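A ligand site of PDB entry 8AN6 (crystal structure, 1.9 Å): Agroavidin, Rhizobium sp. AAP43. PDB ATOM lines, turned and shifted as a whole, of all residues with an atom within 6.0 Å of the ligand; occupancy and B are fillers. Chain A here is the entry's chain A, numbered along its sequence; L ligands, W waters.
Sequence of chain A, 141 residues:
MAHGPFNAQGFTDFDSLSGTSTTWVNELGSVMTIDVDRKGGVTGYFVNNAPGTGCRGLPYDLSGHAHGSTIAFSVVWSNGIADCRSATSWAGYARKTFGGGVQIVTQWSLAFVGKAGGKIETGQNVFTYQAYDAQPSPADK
OG of Ser 30 sits at hydrogen-bond distance from O3 of the ligand, at 2.7 Å. OG of Ser 86 is in hydrogen-bond range of O1 of the ligand (2.8 Å). The side-chain amide oxygen of Asn 48 sits at hydrogen-bond distance from a nitrogen (N2) of the ligand (2.8 Å). N1 of the ligand lies within hydrogen-bond range of OD1 of Asn 125. ND2 of Asn 26 is in hydrogen-bond range of O3 of the ligand, 2.9 Å away. O2 of the ligand sits at hydrogen-bond distance from N of Gly 54 (3.1 Å). A sulfur (S1) of the ligand lies close to the side-chain hydroxyl (OG1) of Thr 88 (3.3 Å).
The side-chain hydroxyl (OG) of Ser 30 sits close to the side-chain amide oxygen (OD1) of Asn 48, 3.4 Å away. The side-chain hydroxyl of Ser 30 sits at hydrogen-bond distance from the backbone NH of Asn 49, 3.1 Å away. The backbone carbonyl oxygen (O) of Ser 86 lies within hydrogen-bond range of the backbone NH (N) of Trp 77. The side-chain amide nitrogen of Asn 48 lies within hydrogen-bond range of the side-chain hydroxyl of Thr 53 (2.7 Å). The side-chain amide oxygen (OD1) of Asn 48 sits at hydrogen-bond distance from the backbone NH (N) of Ala 50, at 3.0 Å. OD1 of Asn 26 lies close to N of Leu 28, at 3.1 Å. The side-chain hydroxyl (OG1) of Thr 88 lies within hydrogen-bond range of the indole nitrogen (NE1) of Trp 77 (2.9 Å). The side-chain sulfur (SG) of Cys 84 forms a disulfide with the side-chain sulfur (SG) of Cys 55 (2.1 Å).
CD1 of Leu 28 touches N1 of the ligand, 3.5 Å away. CZ of Phe 46 touches O3 of the ligand, 3.6 Å away. Ala 50 touches the ligand (CB to N2, 3.5 Å). Thr 53 touches the ligand (CB to O2, 3.5 Å). Trp 77 touches the ligand. Cys 84 touches the ligand. CZ2 of Trp 90 touches S1 of the ligand, 3.8 Å away. CD2 of Trp 108 touches C7 of the ligand (3.4 Å). Of the 24 residues printed, 15 come within 4 Å of the ligand.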
ATOM      1  N   ASN A  26      15.410 -16.292   5.616  1.00  0.00           N
ATOM      2  CA  ASN A  26      15.644 -17.738   5.860  1.00  0.00           C
ATOM      3  C   ASN A  26      14.605 -18.197   6.862  1.00  0.00           C
ATOM      4  O   ASN A  26      13.864 -17.335   7.394  1.00  0.00           O
ATOM      5  CB  ASN A  26      17.100 -18.084   6.210  1.00  0.00           C
ATOM      6  CG  ASN A  26      17.591 -17.613   7.570  1.00  0.00           C
ATOM      7  OD1 ASN A  26      16.823 -17.268   8.457  1.00  0.00           O
ATOM      8  ND2 ASN A  26      18.892 -17.608   7.749  1.00  0.00           N
ATOM      9  N   LEU A  28      14.820 -19.305   9.783  1.00  0.00           N
ATOM     10  CA  LEU A  28      15.061 -18.887  11.186  1.00  0.00           C
ATOM     11  C   LEU A  28      14.614 -17.453  11.398  1.00  0.00           C
ATOM     12  O   LEU A  28      14.727 -16.996  12.546  1.00  0.00           O
ATOM     13  CB  LEU A  28      16.547 -19.023  11.537  1.00  0.00           C
ATOM     14  CG  LEU A  28      17.109 -20.438  11.487  1.00  0.00           C
ATOM     15  CD1 LEU A  28      18.564 -20.402  11.887  1.00  0.00           C
ATOM     16  CD2 LEU A  28      16.300 -21.408  12.351  1.00  0.00           C
ATOM     17  N   GLY A  29      14.155 -16.782  10.349  1.00  0.00           N
ATOM     18  CA  GLY A  29      13.581 -15.430  10.434  1.00  0.00           C
ATOM     19  C   GLY A  29      14.596 -14.334  10.176  1.00  0.00           C
ATOM     20  O   GLY A  29      14.270 -13.155  10.369  1.00  0.00           O
ATOM     21  N   SER A  30      15.805 -14.702   9.748  1.00  0.00           N
ATOM     22  CA  SER A  30      16.887 -13.717   9.510  1.00  0.00           C
ATOM     23  C   SER A  30      16.666 -13.052   8.144  1.00  0.00           C
ATOM     24  O   SER A  30      16.118 -13.692   7.263  1.00  0.00           O
ATOM     25  CB  SER A  30      18.234 -14.387   9.615  1.00  0.00           C
ATOM     26  OG  SER A  30      18.431 -14.876  10.937  1.00  0.00           O
ATOM     27  N   PHE A  46      23.244  -8.230   7.150  1.00  0.00           N
ATOM     28  CA  PHE A  46      22.530  -9.406   7.652  1.00  0.00           C
ATOM     29  C   PHE A  46      21.939  -9.020   8.992  1.00  0.00           C
ATOM     30  O   PHE A  46      22.691  -8.415   9.766  1.00  0.00           O
ATOM     31  CB  PHE A  46      23.505 -10.563   7.777  1.00  0.00           C
ATOM     32  CG  PHE A  46      22.847 -11.905   7.917  1.00  0.00           C
ATOM     33  CD1 PHE A  46      22.264 -12.277   9.108  1.00  0.00           C
ATOM     34  CD2 PHE A  46      22.800 -12.783   6.836  1.00  0.00           C
ATOM     35  CE1 PHE A  46      21.693 -13.535   9.237  1.00  0.00           C
ATOM     36  CE2 PHE A  46      22.195 -14.027   6.967  1.00  0.00           C
ATOM     37  CZ  PHE A  46      21.649 -14.391   8.159  1.00  0.00           C
ATOM     38  N   VAL A  47      20.668  -9.352   9.214  1.00  0.00           N
ATOM     39  CA  VAL A  47      19.945  -9.138  10.502  1.00  0.00           C
ATOM     40  C   VAL A  47      19.476 -10.516  10.957  1.00  0.00           C
ATOM     41  O   VAL A  47      18.615 -11.138  10.284  1.00  0.00           O
ATOM     42  CB  VAL A  47      18.771  -8.142  10.385  1.00  0.00           C
ATOM     43  CG1 VAL A  47      18.292  -7.736  11.765  1.00  0.00           C
ATOM     44  CG2 VAL A  47      19.145  -6.924   9.568  1.00  0.00           C
ATOM     45  N   ASN A  48      20.101 -10.994  12.027  1.00  0.00           N
ATOM     46  CA  ASN A  48      19.846 -12.333  12.621  1.00  0.00           C
ATOM     47  C   ASN A  48      18.606 -12.210  13.492  1.00  0.00           C
ATOM     48  O   ASN A  48      18.503 -11.227  14.243  1.00  0.00           O
ATOM     49  CB  ASN A  48      21.067 -12.776  13.444  1.00  0.00           C
ATOM     50  CG  ASN A  48      20.785 -14.003  14.283  1.00  0.00           C
ATOM     51  OD1 ASN A  48      20.279 -15.007  13.766  1.00  0.00           O
ATOM     52  ND2 ASN A  48      21.129 -13.956  15.545  1.00  0.00           N
ATOM     53  N   ASN A  49      17.696 -13.186  13.410  1.00  0.00           N
ATOM     54  CA  ASN A  49      16.610 -13.325  14.411  1.00  0.00           C
ATOM     55  C   ASN A  49      16.435 -14.796  14.804  1.00  0.00           C
ATOM     56  O   ASN A  49      15.322 -15.152  15.214  1.00  0.00           O
ATOM     57  CB  ASN A  49      15.306 -12.739  13.901  1.00  0.00           C
ATOM     58  CG  ASN A  49      14.333 -12.477  15.030  1.00  0.00           C
ATOM     59  OD1 ASN A  49      14.735 -12.241  16.172  1.00  0.00           O
ATOM     60  ND2 ASN A  49      13.052 -12.561  14.717  1.00  0.00           N
ATOM     61  N   ALA A  50      17.474 -15.625  14.676  1.00  0.00           N
ATOM     62  CA  ALA A  50      17.367 -17.070  14.981  1.00  0.00           C
ATOM     63  C   ALA A  50      17.100 -17.232  16.479  1.00  0.00           C
ATOM     64  O   ALA A  50      17.864 -16.702  17.281  1.00  0.00           O
ATOM     65  CB  ALA A  50      18.618 -17.816  14.578  1.00  0.00           C
ATOM     66  N   GLY A  52      17.404 -18.527  20.156  1.00  0.00           N
ATOM     67  CA  GLY A  52      18.521 -19.068  20.954  1.00  0.00           C
ATOM     68  C   GLY A  52      19.870 -18.443  20.621  1.00  0.00           C
ATOM     69  O   GLY A  52      20.877 -18.951  21.129  1.00  0.00           O
ATOM     70  N   THR A  53      19.956 -17.397  19.801  1.00  0.00           N
ATOM     71  CA  THR A  53      21.279 -16.865  19.368  1.00  0.00           C
ATOM     72  C   THR A  53      21.437 -15.443  19.917  1.00  0.00           C
ATOM     73  O   THR A  53      20.441 -14.883  20.306  1.00  0.00           O
ATOM     74  CB  THR A  53      21.430 -16.975  17.847  1.00  0.00           C
ATOM     75  OG1 THR A  53      20.564 -16.043  17.221  1.00  0.00           O
ATOM     76  CG2 THR A  53      21.142 -18.368  17.333  1.00  0.00           C
ATOM     77  N   GLY A  54      22.652 -14.901  19.931  1.00  0.00           N
ATOM     78  CA  GLY A  54      22.916 -13.496  20.286  1.00  0.00           C
ATOM     79  C   GLY A  54      22.801 -12.601  19.064  1.00  0.00           C
ATOM     80  O   GLY A  54      22.591 -13.137  17.967  1.00  0.00           O
ATOM     81  N   CYS A  55      22.973 -11.288  19.229  1.00  0.00           N
ATOM     82  CA  CYS A  55      23.119 -10.312  18.124  1.00  0.00           C
ATOM     83  C   CYS A  55      21.894 -10.391  17.216  1.00  0.00           C
ATOM     84  O   CYS A  55      22.043 -10.465  15.986  1.00  0.00           O
ATOM     85  CB  CYS A  55      24.419 -10.583  17.371  1.00  0.00           C
ATOM     86  SG  CYS A  55      25.909 -10.306  18.378  1.00  0.00           S
ATOM     87  N   TRP A  77      30.028 -11.296  13.555  1.00  0.00           N
ATOM     88  CA  TRP A  77      28.979 -10.802  14.485  1.00  0.00           C
ATOM     89  C   TRP A  77      29.536  -9.740  15.414  1.00  0.00           C
ATOM     90  O   TRP A  77      29.428  -9.916  16.647  1.00  0.00           O
ATOM     91  CB  TRP A  77      28.414 -11.986  15.260  1.00  0.00           C
ATOM     92  CG  TRP A  77      27.795 -12.948  14.317  1.00  0.00           C
ATOM     93  CD1 TRP A  77      28.279 -14.153  13.897  1.00  0.00           C
ATOM     94  CD2 TRP A  77      26.608 -12.703  13.551  1.00  0.00           C
ATOM     95  NE1 TRP A  77      27.428 -14.710  12.986  1.00  0.00           N
ATOM     96  CE2 TRP A  77      26.406 -13.836  12.732  1.00  0.00           C
ATOM     97  CE3 TRP A  77      25.716 -11.642  13.484  1.00  0.00           C
ATOM     98  CZ2 TRP A  77      25.305 -13.944  11.905  1.00  0.00           C
ATOM     99  CZ3 TRP A  77      24.615 -11.749  12.658  1.00  0.00           C
ATOM    100  CH2 TRP A  77      24.422 -12.879  11.864  1.00  0.00           C
ATOM    101  N   CYS A  84      29.107 -10.626  19.405  1.00  0.00           N
ATOM    102  CA  CYS A  84      28.905 -12.037  19.853  1.00  0.00           C
ATOM    103  C   CYS A  84      30.209 -12.848  19.742  1.00  0.00           C
ATOM    104  O   CYS A  84      30.160 -14.009  20.073  1.00  0.00           O
ATOM    105  CB  CYS A  84      27.754 -12.685  19.098  1.00  0.00           C
ATOM    106  SG  CYS A  84      26.144 -11.976  19.557  1.00  0.00           S
ATOM    107  N   ARG A  85      31.342 -12.233  19.412  1.00  0.00           N
ATOM    108  CA  ARG A  85      32.675 -12.895  19.317  1.00  0.00           C
ATOM    109  C   ARG A  85      32.565 -14.159  18.444  1.00  0.00           C
ATOM    110  O   ARG A  85      33.085 -15.225  18.833  1.00  0.00           O
ATOM    111  CB  ARG A  85      33.191 -13.286  20.703  1.00  0.00           C
ATOM    112  CG  ARG A  85      33.695 -12.120  21.524  1.00  0.00           C
ATOM    113  CD  ARG A  85      33.350 -12.337  22.989  1.00  0.00           C
ATOM    114  NE  ARG A  85      34.092 -11.417  23.841  1.00  0.00           N
ATOM    115  CZ  ARG A  85      33.787 -11.136  25.108  1.00  0.00           C
ATOM    116  NH1 ARG A  85      34.522 -10.273  25.780  1.00  0.00           N
ATOM    117  NH2 ARG A  85      32.747 -11.710  25.687  1.00  0.00           N
ATOM    118  N   SER A  86      31.867 -14.059  17.311  1.00  0.00           N
ATOM    119  CA  SER A  86      31.610 -15.219  16.431  1.00  0.00           C
ATOM    120  C   SER A  86      31.592 -14.771  14.982  1.00  0.00           C
ATOM    121  O   SER A  86      31.549 -13.575  14.725  1.00  0.00           O
ATOM    122  CB  SER A  86      30.352 -15.918  16.839  1.00  0.00           C
ATOM    123  OG  SER A  86      29.285 -14.991  16.873  1.00  0.00           O
ATOM    124  N   THR A  88      30.077 -16.256  10.940  1.00  0.00           N
ATOM    125  CA  THR A  88      29.352 -17.263  10.124  1.00  0.00           C
ATOM    126  C   THR A  88      29.718 -17.067   8.654  1.00  0.00           C
ATOM    127  O   THR A  88      29.808 -15.911   8.165  1.00  0.00           O
ATOM    128  CB  THR A  88      27.846 -17.199  10.379  1.00  0.00           C
ATOM    129  OG1 THR A  88      27.642 -17.323  11.783  1.00  0.00           O
ATOM    130  CG2 THR A  88      27.104 -18.296   9.656  1.00  0.00           C
ATOM    131  N   TRP A  90      28.379 -18.868   4.824  1.00  0.00           N
ATOM    132  CA  TRP A  90      27.362 -19.662   4.100  1.00  0.00           C
ATOM    133  C   TRP A  90      27.914 -19.945   2.708  1.00  0.00           C
ATOM    134  O   TRP A  90      28.574 -19.059   2.171  1.00  0.00           O
ATOM    135  CB  TRP A  90      26.055 -18.875   3.996  1.00  0.00           C
ATOM    136  CG  TRP A  90      25.241 -18.691   5.244  1.00  0.00           C
ATOM    137  CD1 TRP A  90      24.137 -19.411   5.600  1.00  0.00           C
ATOM    138  CD2 TRP A  90      25.377 -17.655   6.221  1.00  0.00           C
ATOM    139  NE1 TRP A  90      23.604 -18.920   6.763  1.00  0.00           N
ATOM    140  CE2 TRP A  90      24.329 -17.827   7.159  1.00  0.00           C
ATOM    141  CE3 TRP A  90      26.268 -16.590   6.396  1.00  0.00           C
ATOM    142  CZ2 TRP A  90      24.158 -16.989   8.255  1.00  0.00           C
ATOM    143  CZ3 TRP A  90      26.078 -15.754   7.461  1.00  0.00           C
ATOM    144  CH2 TRP A  90      25.052 -15.960   8.389  1.00  0.00           C
ATOM    145  N   TRP A 108      25.800 -23.457   6.596  1.00  0.00           N
ATOM    146  CA  TRP A 108      26.502 -22.415   7.385  1.00  0.00           C
ATOM    147  C   TRP A 108      27.436 -23.127   8.346  1.00  0.00           C
ATOM    148  O   TRP A 108      27.152 -24.292   8.715  1.00  0.00           O
ATOM    149  CB  TRP A 108      25.550 -21.441   8.092  1.00  0.00           C
ATOM    150  CG  TRP A 108      24.527 -22.057   8.994  1.00  0.00           C
ATOM    151  CD1 TRP A 108      23.248 -22.370   8.658  1.00  0.00           C
ATOM    152  CD2 TRP A 108      24.686 -22.438  10.369  1.00  0.00           C
ATOM    153  NE1 TRP A 108      22.595 -22.888   9.741  1.00  0.00           N
ATOM    154  CE2 TRP A 108      23.448 -22.948  10.806  1.00  0.00           C
ATOM    155  CE3 TRP A 108      25.757 -22.394  11.283  1.00  0.00           C
ATOM    156  CZ2 TRP A 108      23.233 -23.410  12.098  1.00  0.00           C
ATOM    157  CZ3 TRP A 108      25.538 -22.858  12.561  1.00  0.00           C
ATOM    158  CH2 TRP A 108      24.298 -23.353  12.967  1.00  0.00           C
ATOM    159  N   LEU A 110      29.381 -21.728  11.943  1.00  0.00           N
ATOM    160  CA  LEU A 110      29.514 -20.677  12.972  1.00  0.00           C
ATOM    161  C   LEU A 110      30.700 -21.040  13.874  1.00  0.00           C
ATOM    162  O   LEU A 110      30.664 -22.118  14.530  1.00  0.00           O
ATOM    163  CB  LEU A 110      28.193 -20.613  13.751  1.00  0.00           C
ATOM    164  CG  LEU A 110      28.171 -19.785  15.037  1.00  0.00           C
ATOM    165  CD1 LEU A 110      28.818 -18.426  14.861  1.00  0.00           C
ATOM    166  CD2 LEU A 110      26.715 -19.613  15.479  1.00  0.00           C
ATOM    167  N   PHE A 112      33.281 -19.764  17.042  1.00  0.00           N
ATOM    168  CA  PHE A 112      33.437 -18.976  18.284  1.00  0.00           C
ATOM    169  C   PHE A 112      34.438 -19.724  19.172  1.00  0.00           C
ATOM    170  O   PHE A 112      34.711 -20.932  18.957  1.00  0.00           O
ATOM    171  CB  PHE A 112      32.080 -18.812  18.965  1.00  0.00           C
ATOM    172  CG  PHE A 112      31.456 -20.111  19.397  1.00  0.00           C
ATOM    173  CD1 PHE A 112      30.723 -20.881  18.494  1.00  0.00           C
ATOM    174  CD2 PHE A 112      31.626 -20.599  20.684  1.00  0.00           C
ATOM    175  CE1 PHE A 112      30.168 -22.097  18.883  1.00  0.00           C
ATOM    176  CE2 PHE A 112      31.058 -21.808  21.077  1.00  0.00           C
ATOM    177  CZ  PHE A 112      30.333 -22.548  20.174  1.00  0.00           C
ATOM    178  N   ASN A 125      20.526 -23.439   6.080  1.00  0.00           N
ATOM    179  CA  ASN A 125      19.517 -22.368   5.955  1.00  0.00           C
ATOM    180  C   ASN A 125      19.013 -22.440   4.526  1.00  0.00           C
ATOM    181  O   ASN A 125      19.813 -22.767   3.633  1.00  0.00           O
ATOM    182  CB  ASN A 125      20.049 -20.973   6.269  1.00  0.00           C
ATOM    183  CG  ASN A 125      20.285 -20.683   7.728  1.00  0.00           C
ATOM    184  OD1 ASN A 125      21.050 -19.782   8.052  1.00  0.00           O
ATOM    185  ND2 ASN A 125      19.637 -21.397   8.631  1.00  0.00           N
ATOM    186  N   PHE A 127      17.344 -19.562   2.184  1.00  0.00           N
ATOM    187  CA  PHE A 127      16.910 -18.162   2.002  1.00  0.00           C
ATOM    188  C   PHE A 127      15.874 -18.103   0.866  1.00  0.00           C
ATOM    189  O   PHE A 127      16.024 -18.791  -0.165  1.00  0.00           O
ATOM    190  CB  PHE A 127      18.111 -17.247   1.731  1.00  0.00           C
ATOM    191  CG  PHE A 127      19.092 -17.225   2.876  1.00  0.00           C
ATOM    192  CD1 PHE A 127      19.981 -18.264   3.062  1.00  0.00           C
ATOM    193  CD2 PHE A 127      19.096 -16.171   3.761  1.00  0.00           C
ATOM    194  CE1 PHE A 127      20.892 -18.242   4.103  1.00  0.00           C
ATOM    195  CE2 PHE A 127      19.975 -16.162   4.830  1.00  0.00           C
ATOM    196  CZ  PHE A 127      20.879 -17.191   4.995  1.00  0.00           C
HETATM  197  C1  LIG L   1      25.834 -15.797  17.757  1.00  0.00           C
HETATM  198  O1  LIG L   1      27.013 -16.132  18.060  1.00  0.00           O
HETATM  199  O2  LIG L   1      24.813 -16.322  18.262  1.00  0.00           O
HETATM  200  C2  LIG L   1      25.633 -14.718  16.709  1.00  0.00           C
HETATM  201  C3  LIG L   1      24.454 -14.959  15.813  1.00  0.00           C
HETATM  202  C4  LIG L   1      24.512 -16.245  15.026  1.00  0.00           C
HETATM  203  C5  LIG L   1      23.301 -16.484  14.127  1.00  0.00           C
HETATM  204  C6  LIG L   1      23.265 -17.847  13.451  1.00  0.00           C
HETATM  205  S1  LIG L   1      24.350 -17.766  11.989  1.00  0.00           S
HETATM  206  C7  LIG L   1      23.641 -19.364  11.522  1.00  0.00           C
HETATM  207  C8  LIG L   1      22.130 -19.289  11.770  1.00  0.00           C
HETATM  208  N1  LIG L   1      21.397 -18.710  10.665  1.00  0.00           N
HETATM  209  C9  LIG L   1      20.848 -17.528  10.982  1.00  0.00           C
HETATM  210  O3  LIG L   1      20.126 -16.832  10.243  1.00  0.00           O
HETATM  211  N2  LIG L   1      21.181 -17.229  12.254  1.00  0.00           N
HETATM  212  C10 LIG L   1      21.886 -18.283  12.923  1.00  0.00           C
HETATM  213  O   HOH W   1      27.767 -17.915  19.644  1.00  0.00           O
